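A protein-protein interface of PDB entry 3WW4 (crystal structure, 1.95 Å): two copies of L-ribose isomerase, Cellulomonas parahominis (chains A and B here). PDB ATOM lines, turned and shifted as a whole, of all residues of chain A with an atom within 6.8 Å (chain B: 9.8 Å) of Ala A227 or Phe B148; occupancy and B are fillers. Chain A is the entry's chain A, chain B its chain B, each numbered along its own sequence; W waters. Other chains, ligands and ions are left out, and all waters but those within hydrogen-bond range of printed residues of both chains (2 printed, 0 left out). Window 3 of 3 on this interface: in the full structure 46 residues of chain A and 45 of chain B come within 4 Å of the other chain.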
ATOM      1  N   GLU A  78     -11.552   9.648  -6.768  1.00  0.00           N
ATOM      2  CA  GLU A  78     -10.473  10.555  -7.121  1.00  0.00           C
ATOM      3  C   GLU A  78      -9.097   9.873  -7.076  1.00  0.00           C
ATOM      4  O   GLU A  78      -8.677   9.359  -6.039  1.00  0.00           O
ATOM      5  CB  GLU A  78     -10.511  11.731  -6.135  1.00  0.00           C
ATOM      6  CG  GLU A  78      -9.323  12.663  -6.164  1.00  0.00           C
ATOM      7  CD  GLU A  78      -9.118  13.296  -7.525  1.00  0.00           C
ATOM      8  OE1 GLU A  78     -10.109  13.786  -8.113  1.00  0.00           O
ATOM      9  OE2 GLU A  78      -7.964  13.306  -7.996  1.00  0.00           O
ATOM     10  N   PRO A  79      -8.375   9.863  -8.206  1.00  0.00           N
ATOM     11  CA  PRO A  79      -7.052   9.237  -8.249  1.00  0.00           C
ATOM     12  C   PRO A  79      -6.059   9.894  -7.294  1.00  0.00           C
ATOM     13  O   PRO A  79      -5.127   9.243  -6.809  1.00  0.00           O
ATOM     14  CB  PRO A  79      -6.646   9.404  -9.707  1.00  0.00           C
ATOM     15  CG  PRO A  79      -7.963   9.375 -10.426  1.00  0.00           C
ATOM     16  CD  PRO A  79      -8.811  10.254  -9.559  1.00  0.00           C
ATOM     17  N   ALA A  80      -6.266  11.183  -7.029  1.00  0.00           N
ATOM     18  CA  ALA A  80      -5.395  11.958  -6.145  1.00  0.00           C
ATOM     19  C   ALA A  80      -3.943  11.884  -6.599  1.00  0.00           C
ATOM     20  O   ALA A  80      -3.018  11.922  -5.789  1.00  0.00           O
ATOM     21  CB  ALA A  80      -5.521  11.474  -4.701  1.00  0.00           C
ATOM     22  N   VAL A  81      -3.754  11.781  -7.906  1.00  0.00           N
ATOM     23  CA  VAL A  81      -2.427  11.714  -8.494  1.00  0.00           C
ATOM     24  C   VAL A  81      -1.874  13.122  -8.733  1.00  0.00           C
ATOM     25  O   VAL A  81      -0.661  13.333  -8.734  1.00  0.00           O
ATOM     26  CB  VAL A  81      -2.480  10.926  -9.809  1.00  0.00           C
ATOM     27  CG1 VAL A  81      -1.242  11.171 -10.621  1.00  0.00           C
ATOM     28  CG2 VAL A  81      -2.616   9.438  -9.496  1.00  0.00           C
ATOM     29  N   ASP A  82      -2.766  14.091  -8.918  1.00  0.00           N
ATOM     30  CA  ASP A  82      -2.330  15.463  -9.142  1.00  0.00           C
ATOM     31  C   ASP A  82      -1.511  15.994  -7.970  1.00  0.00           C
ATOM     32  O   ASP A  82      -1.955  15.946  -6.811  1.00  0.00           O
ATOM     33  CB  ASP A  82      -3.530  16.377  -9.375  1.00  0.00           C
ATOM     34  CG  ASP A  82      -4.106  16.231 -10.761  1.00  0.00           C
ATOM     35  OD1 ASP A  82      -4.915  15.300 -10.989  1.00  0.00           O
ATOM     36  OD2 ASP A  82      -3.734  17.049 -11.631  1.00  0.00           O
ATOM     37  N   GLY A  83      -0.312  16.494  -8.280  1.00  0.00           N
ATOM     38  CA  GLY A  83       0.554  17.036  -7.248  1.00  0.00           C
ATOM     39  C   GLY A  83       1.506  16.037  -6.613  1.00  0.00           C
ATOM     40  O   GLY A  83       2.408  16.429  -5.869  1.00  0.00           O
ATOM     41  N   TYR A 215      -8.678   4.726  -3.784  1.00  0.00           N
ATOM     42  CA  TYR A 215      -9.191   4.537  -5.140  1.00  0.00           C
ATOM     43  C   TYR A 215      -9.749   3.152  -5.439  1.00  0.00           C
ATOM     44  O   TYR A 215      -9.153   2.127  -5.104  1.00  0.00           O
ATOM     45  CB  TYR A 215      -8.116   4.869  -6.174  1.00  0.00           C
ATOM     46  CG  TYR A 215      -8.672   5.045  -7.569  1.00  0.00           C
ATOM     47  CD1 TYR A 215      -9.302   6.229  -7.943  1.00  0.00           C
ATOM     48  CD2 TYR A 215      -8.571   4.024  -8.514  1.00  0.00           C
ATOM     49  CE1 TYR A 215      -9.813   6.397  -9.224  1.00  0.00           C
ATOM     50  CE2 TYR A 215      -9.072   4.179  -9.793  1.00  0.00           C
ATOM     51  CZ  TYR A 215      -9.693   5.369 -10.145  1.00  0.00           C
ATOM     52  OH  TYR A 215     -10.184   5.522 -11.422  1.00  0.00           O
ATOM     53  N   ALA A 227      -9.352   7.592 -20.365  1.00  0.00           N
ATOM     54  CA  ALA A 227      -7.985   7.918 -19.970  1.00  0.00           C
ATOM     55  C   ALA A 227      -7.736   7.517 -18.520  1.00  0.00           C
ATOM     56  O   ALA A 227      -8.480   7.912 -17.625  1.00  0.00           O
ATOM     57  CB  ALA A 227      -7.731   9.416 -20.153  1.00  0.00           C
ATOM     58  N   ALA A 228      -6.690   6.725 -18.298  1.00  0.00           N
ATOM     59  CA  ALA A 228      -6.337   6.272 -16.957  1.00  0.00           C
ATOM     60  C   ALA A 228      -5.434   7.299 -16.287  1.00  0.00           C
ATOM     61  O   ALA A 228      -4.598   7.918 -16.940  1.00  0.00           O
ATOM     62  CB  ALA A 228      -5.630   4.921 -17.029  1.00  0.00           C
ATOM     63  N   PRO A 229      -5.591   7.491 -14.969  1.00  0.00           N
ATOM     64  CA  PRO A 229      -4.772   8.457 -14.230  1.00  0.00           C
ATOM     65  C   PRO A 229      -3.289   8.231 -14.516  1.00  0.00           C
ATOM     66  O   PRO A 229      -2.498   9.172 -14.570  1.00  0.00           O
ATOM     67  CB  PRO A 229      -5.127   8.167 -12.775  1.00  0.00           C
ATOM     68  CG  PRO A 229      -6.540   7.686 -12.869  1.00  0.00           C
ATOM     69  CD  PRO A 229      -6.498   6.768 -14.062  1.00  0.00           C
ATOM     70  N   LEU A 230      -2.934   6.965 -14.694  1.00  0.00           N
ATOM     71  CA  LEU A 230      -1.568   6.552 -14.985  1.00  0.00           C
ATOM     72  C   LEU A 230      -1.651   5.343 -15.902  1.00  0.00           C
ATOM     73  O   LEU A 230      -2.587   4.551 -15.806  1.00  0.00           O
ATOM     74  CB  LEU A 230      -0.835   6.172 -13.697  1.00  0.00           C
ATOM     75  CG  LEU A 230      -0.505   7.317 -12.738  1.00  0.00           C
ATOM     76  CD1 LEU A 230       0.127   6.774 -11.470  1.00  0.00           C
ATOM     77  CD2 LEU A 230       0.441   8.282 -13.422  1.00  0.00           C
ATOM     78  N   ARG A 234      -4.423   1.197 -16.217  1.00  0.00           N
ATOM     79  CA  ARG A 234      -5.341   0.657 -17.221  1.00  0.00           C
ATOM     80  C   ARG A 234      -5.675  -0.819 -17.015  1.00  0.00           C
ATOM     81  O   ARG A 234      -4.780  -1.650 -16.854  1.00  0.00           O
ATOM     82  CB  ARG A 234      -4.752   0.819 -18.624  1.00  0.00           C
ATOM     83  CG  ARG A 234      -4.541   2.250 -19.088  1.00  0.00           C
ATOM     84  CD  ARG A 234      -3.838   2.265 -20.446  1.00  0.00           C
ATOM     85  NE  ARG A 234      -4.617   1.570 -21.470  1.00  0.00           N
ATOM     86  CZ  ARG A 234      -4.120   1.125 -22.622  1.00  0.00           C
ATOM     87  NH1 ARG A 234      -2.835   1.296 -22.909  1.00  0.00           N
ATOM     88  NH2 ARG A 234      -4.909   0.508 -23.492  1.00  0.00           N
ATOM     89  N   VAL B 145       6.256  16.467 -10.890  1.00  0.00           N
ATOM     90  CA  VAL B 145       4.972  16.275 -10.237  1.00  0.00           C
ATOM     91  C   VAL B 145       4.021  15.675 -11.260  1.00  0.00           C
ATOM     92  O   VAL B 145       4.090  16.003 -12.442  1.00  0.00           O
ATOM     93  CB  VAL B 145       4.397  17.618  -9.744  1.00  0.00           C
ATOM     94  CG1 VAL B 145       3.006  17.413  -9.193  1.00  0.00           C
ATOM     95  CG2 VAL B 145       5.304  18.210  -8.679  1.00  0.00           C
ATOM     96  N   LEU B 146       3.136  14.794 -10.808  1.00  0.00           N
ATOM     97  CA  LEU B 146       2.184  14.167 -11.711  1.00  0.00           C
ATOM     98  C   LEU B 146       0.994  15.079 -11.986  1.00  0.00           C
ATOM     99  O   LEU B 146       0.716  16.004 -11.220  1.00  0.00           O
ATOM    100  CB  LEU B 146       1.699  12.845 -11.121  1.00  0.00           C
ATOM    101  CG  LEU B 146       2.788  11.796 -10.887  1.00  0.00           C
ATOM    102  CD1 LEU B 146       2.172  10.564 -10.234  1.00  0.00           C
ATOM    103  CD2 LEU B 146       3.442  11.442 -12.213  1.00  0.00           C
ATOM    104  N   SER B 147       0.299  14.809 -13.087  1.00  0.00           N
ATOM    105  CA  SER B 147      -0.865  15.589 -13.492  1.00  0.00           C
ATOM    106  C   SER B 147      -1.925  14.680 -14.094  1.00  0.00           C
ATOM    107  O   SER B 147      -1.607  13.654 -14.697  1.00  0.00           O
ATOM    108  CB  SER B 147      -0.479  16.643 -14.539  1.00  0.00           C
ATOM    109  OG  SER B 147       0.427  17.596 -14.017  1.00  0.00           O
ATOM    110  N   PHE B 148      -3.185  15.063 -13.936  1.00  0.00           N
ATOM    111  CA  PHE B 148      -4.276  14.283 -14.486  1.00  0.00           C
ATOM    112  C   PHE B 148      -5.503  15.150 -14.728  1.00  0.00           C
ATOM    113  O   PHE B 148      -5.934  15.334 -15.868  1.00  0.00           O
ATOM    114  CB  PHE B 148      -4.643  13.130 -13.553  1.00  0.00           C
ATOM    115  CG  PHE B 148      -5.806  12.317 -14.043  1.00  0.00           C
ATOM    116  CD1 PHE B 148      -5.741  11.663 -15.272  1.00  0.00           C
ATOM    117  CD2 PHE B 148      -6.978  12.230 -13.295  1.00  0.00           C
ATOM    118  CE1 PHE B 148      -6.831  10.933 -15.753  1.00  0.00           C
ATOM    119  CE2 PHE B 148      -8.077  11.501 -13.768  1.00  0.00           C
ATOM    120  CZ  PHE B 148      -8.000  10.852 -14.999  1.00  0.00           C
ATOM    121  N   SER B 149      -6.067  15.670 -13.644  1.00  0.00           N
ATOM    122  CA  SER B 149      -7.240  16.516 -13.731  1.00  0.00           C
ATOM    123  C   SER B 149      -7.008  17.772 -12.908  1.00  0.00           C
ATOM    124  O   SER B 149      -7.354  17.829 -11.730  1.00  0.00           O
ATOM    125  CB  SER B 149      -8.470  15.772 -13.214  1.00  0.00           C
ATOM    126  OG  SER B 149      -8.293  15.388 -11.866  1.00  0.00           O
ATOM    127  N   PRO B 150      -6.410  18.799 -13.524  1.00  0.00           N
ATOM    128  CA  PRO B 150      -6.125  20.067 -12.847  1.00  0.00           C
ATOM    129  C   PRO B 150      -7.378  20.756 -12.309  1.00  0.00           C
ATOM    130  O   PRO B 150      -8.498  20.441 -12.712  1.00  0.00           O
ATOM    131  CB  PRO B 150      -5.425  20.882 -13.930  1.00  0.00           C
ATOM    132  CG  PRO B 150      -6.045  20.364 -15.186  1.00  0.00           C
ATOM    133  CD  PRO B 150      -6.053  18.875 -14.948  1.00  0.00           C
ATOM    134  N   MET B 151      -7.177  21.692 -11.390  1.00  0.00           N
ATOM    135  CA  MET B 151      -8.276  22.426 -10.778  1.00  0.00           C
ATOM    136  C   MET B 151      -9.029  23.279 -11.780  1.00  0.00           C
ATOM    137  O   MET B 151      -8.426  23.919 -12.641  1.00  0.00           O
ATOM    138  CB  MET B 151      -7.751  23.341  -9.668  1.00  0.00           C
ATOM    139  CG  MET B 151      -7.198  22.612  -8.462  1.00  0.00           C
ATOM    140  SD  MET B 151      -8.472  21.669  -7.623  1.00  0.00           S
ATOM    141  CE  MET B 151      -9.265  22.978  -6.683  1.00  0.00           C
ATOM    142  N   VAL B 188     -13.320  18.622  -5.315  1.00  0.00           N
ATOM    143  CA  VAL B 188     -11.956  18.268  -4.947  1.00  0.00           C
ATOM    144  C   VAL B 188     -10.937  19.408  -4.921  1.00  0.00           C
ATOM    145  O   VAL B 188     -10.877  20.246  -5.829  1.00  0.00           O
ATOM    146  CB  VAL B 188     -11.431  17.151  -5.872  1.00  0.00           C
ATOM    147  CG1 VAL B 188      -9.988  16.792  -5.512  1.00  0.00           C
ATOM    148  CG2 VAL B 188     -12.327  15.915  -5.743  1.00  0.00           C
ATOM    149  N   HIS B 190      -7.103  19.601  -4.819  1.00  0.00           N
ATOM    150  CA  HIS B 190      -5.829  18.915  -4.933  1.00  0.00           C
ATOM    151  C   HIS B 190      -4.765  19.546  -4.050  1.00  0.00           C
ATOM    152  O   HIS B 190      -4.779  20.753  -3.799  1.00  0.00           O
ATOM    153  CB  HIS B 190      -5.354  18.938  -6.384  1.00  0.00           C
ATOM    154  CG  HIS B 190      -6.197  18.114  -7.304  1.00  0.00           C
ATOM    155  ND1 HIS B 190      -6.421  16.769  -7.100  1.00  0.00           N
ATOM    156  CD2 HIS B 190      -6.852  18.437  -8.444  1.00  0.00           C
ATOM    157  CE1 HIS B 190      -7.177  16.299  -8.075  1.00  0.00           C
ATOM    158  NE2 HIS B 190      -7.452  17.290  -8.904  1.00  0.00           N
ATOM    159  N   ARG B 191      -3.852  18.708  -3.577  1.00  0.00           N
ATOM    160  CA  ARG B 191      -2.741  19.141  -2.745  1.00  0.00           C
ATOM    161  C   ARG B 191      -1.935  20.209  -3.498  1.00  0.00           C
ATOM    162  O   ARG B 191      -1.985  20.286  -4.732  1.00  0.00           O
ATOM    163  CB  ARG B 191      -1.841  17.943  -2.437  1.00  0.00           C
ATOM    164  CG  ARG B 191      -1.363  17.219  -3.692  1.00  0.00           C
ATOM    165  CD  ARG B 191      -0.315  16.164  -3.370  1.00  0.00           C
ATOM    166  NE  ARG B 191      -0.880  14.958  -2.776  1.00  0.00           N
ATOM    167  CZ  ARG B 191      -1.494  13.993  -3.460  1.00  0.00           C
ATOM    168  NH1 ARG B 191      -1.634  14.084  -4.778  1.00  0.00           N
ATOM    169  NH2 ARG B 191      -1.951  12.923  -2.826  1.00  0.00           N
ATOM    170  N   HIS B 193      -2.446  23.341  -3.535  1.00  0.00           N
ATOM    171  CA  HIS B 193      -3.284  24.450  -3.962  1.00  0.00           C
ATOM    172  C   HIS B 193      -3.675  25.282  -2.756  1.00  0.00           C
ATOM    173  O   HIS B 193      -4.149  24.739  -1.759  1.00  0.00           O
ATOM    174  CB  HIS B 193      -4.559  23.928  -4.634  1.00  0.00           C
ATOM    175  CG  HIS B 193      -4.362  23.468  -6.044  1.00  0.00           C
ATOM    176  ND1 HIS B 193      -4.471  24.315  -7.125  1.00  0.00           N
ATOM    177  CD2 HIS B 193      -4.064  22.248  -6.549  1.00  0.00           C
ATOM    178  CE1 HIS B 193      -4.252  23.637  -8.238  1.00  0.00           C
ATOM    179  NE2 HIS B 193      -4.004  22.380  -7.916  1.00  0.00           N
HETATM  180  O   HOH W   1      -1.730  10.011  -3.473  1.00  0.00           O
HETATM  181  O   HOH W   2      -4.486  15.187  -5.890  1.00  0.00           O
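The backbone NH (N) of His B190 lies close to the side-chain sulfur (SD) of Met B151, at 3.7 Å. The backbone NH of Ala A80 is in hydrogen-bond range of the side-chain carboxylate of Glu A78. O of Ser B149 is in hydrogen-bond range of NE2 of His B190 (2.9 Å).
No position is printed for both chains.
Among the printed residues, merely in contact across the chains: Glu A78 with Val B188 (3.9 Å), Glu A78 with His B190 (3.1 Å), Pro A79 with Phe B148 (3.96 Å), Val A81 with Leu B146 (3.4 Å), Asp A82 with Leu B146 (3.7 Å), Asp A82 with Ser B147 (3.7 Å), Asp A82 with Pro B150 (3.7 Å), Asp A82 with His B190 (3.7 Å), Gly A83 with Val B145 (3.2 Å), Gly A83 with Arg B191 (3.7 Å), Ala A227 with Phe B148 (3.9 Å), Ala A228 with Phe B148 (3.9 Å) and Pro A229 with Phe B148 (3.5 Å).
Hydrophobic or aromatic side chains of chain A within 4 Å of the printed part of chain B: Pro A79 and Val A81. Among the printed residues, 18 pairs touch across the chains.
Ala A227 touches just one residue of chain B: Phe B148. Of the printed residues of chain A, Phe B148 touches Pro A79 (3.96 Å), Asp A82 (3.1 Å), Ala A227 (3.9 Å), Ala A228 (3.9 Å) and Pro A229 (3.5 Å). Printed residues of chain B within 4 Å of Ala A228: Phe B148. Pro A229 touches just one residue of chain B: Phe B148. Of the printed residues of chain B, Val A81 touches Leu B146. Printed residues of chain B within 4 Å of Ala A80: Arg B191 (2.8 Å). Of the printed residues of chain B, Glu A78 touches Val B188 and His B190.
Water W2 lies within hydrogen-bond range of a ring nitrogen (ND1) of His B190 (2.8 Å), the backbone carbonyl oxygen of Asp A82 (2.8 Å) and the guanidinium group of Arg B191 (3.3 Å). Water W1 bridges the guanidinium group of Arg B191 (3.0 Å) and the backbone carbonyl oxygen of Ala A80 (3.3 Å).
The backbone NH (N) of Gly A83 is in hydrogen-bond range of the backbone carbonyl oxygen (O) of Leu B146. The side-chain carboxylate of Asp A82 lies within hydrogen-bond range of the backbone NH of Phe B148 (3.1 Å). The backbone carbonyl oxygen (O) of Asp A82 lies within hydrogen-bond range of the guanidinium group (NH1) of Arg B191, at 2.8 Å. The side-chain carboxylate of Asp A82 is in hydrogen-bond range of the backbone NH of Ser B149. NH1 of Arg B191 lies within hydrogen-bond range of O of Ala A80, at 2.8 Å.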
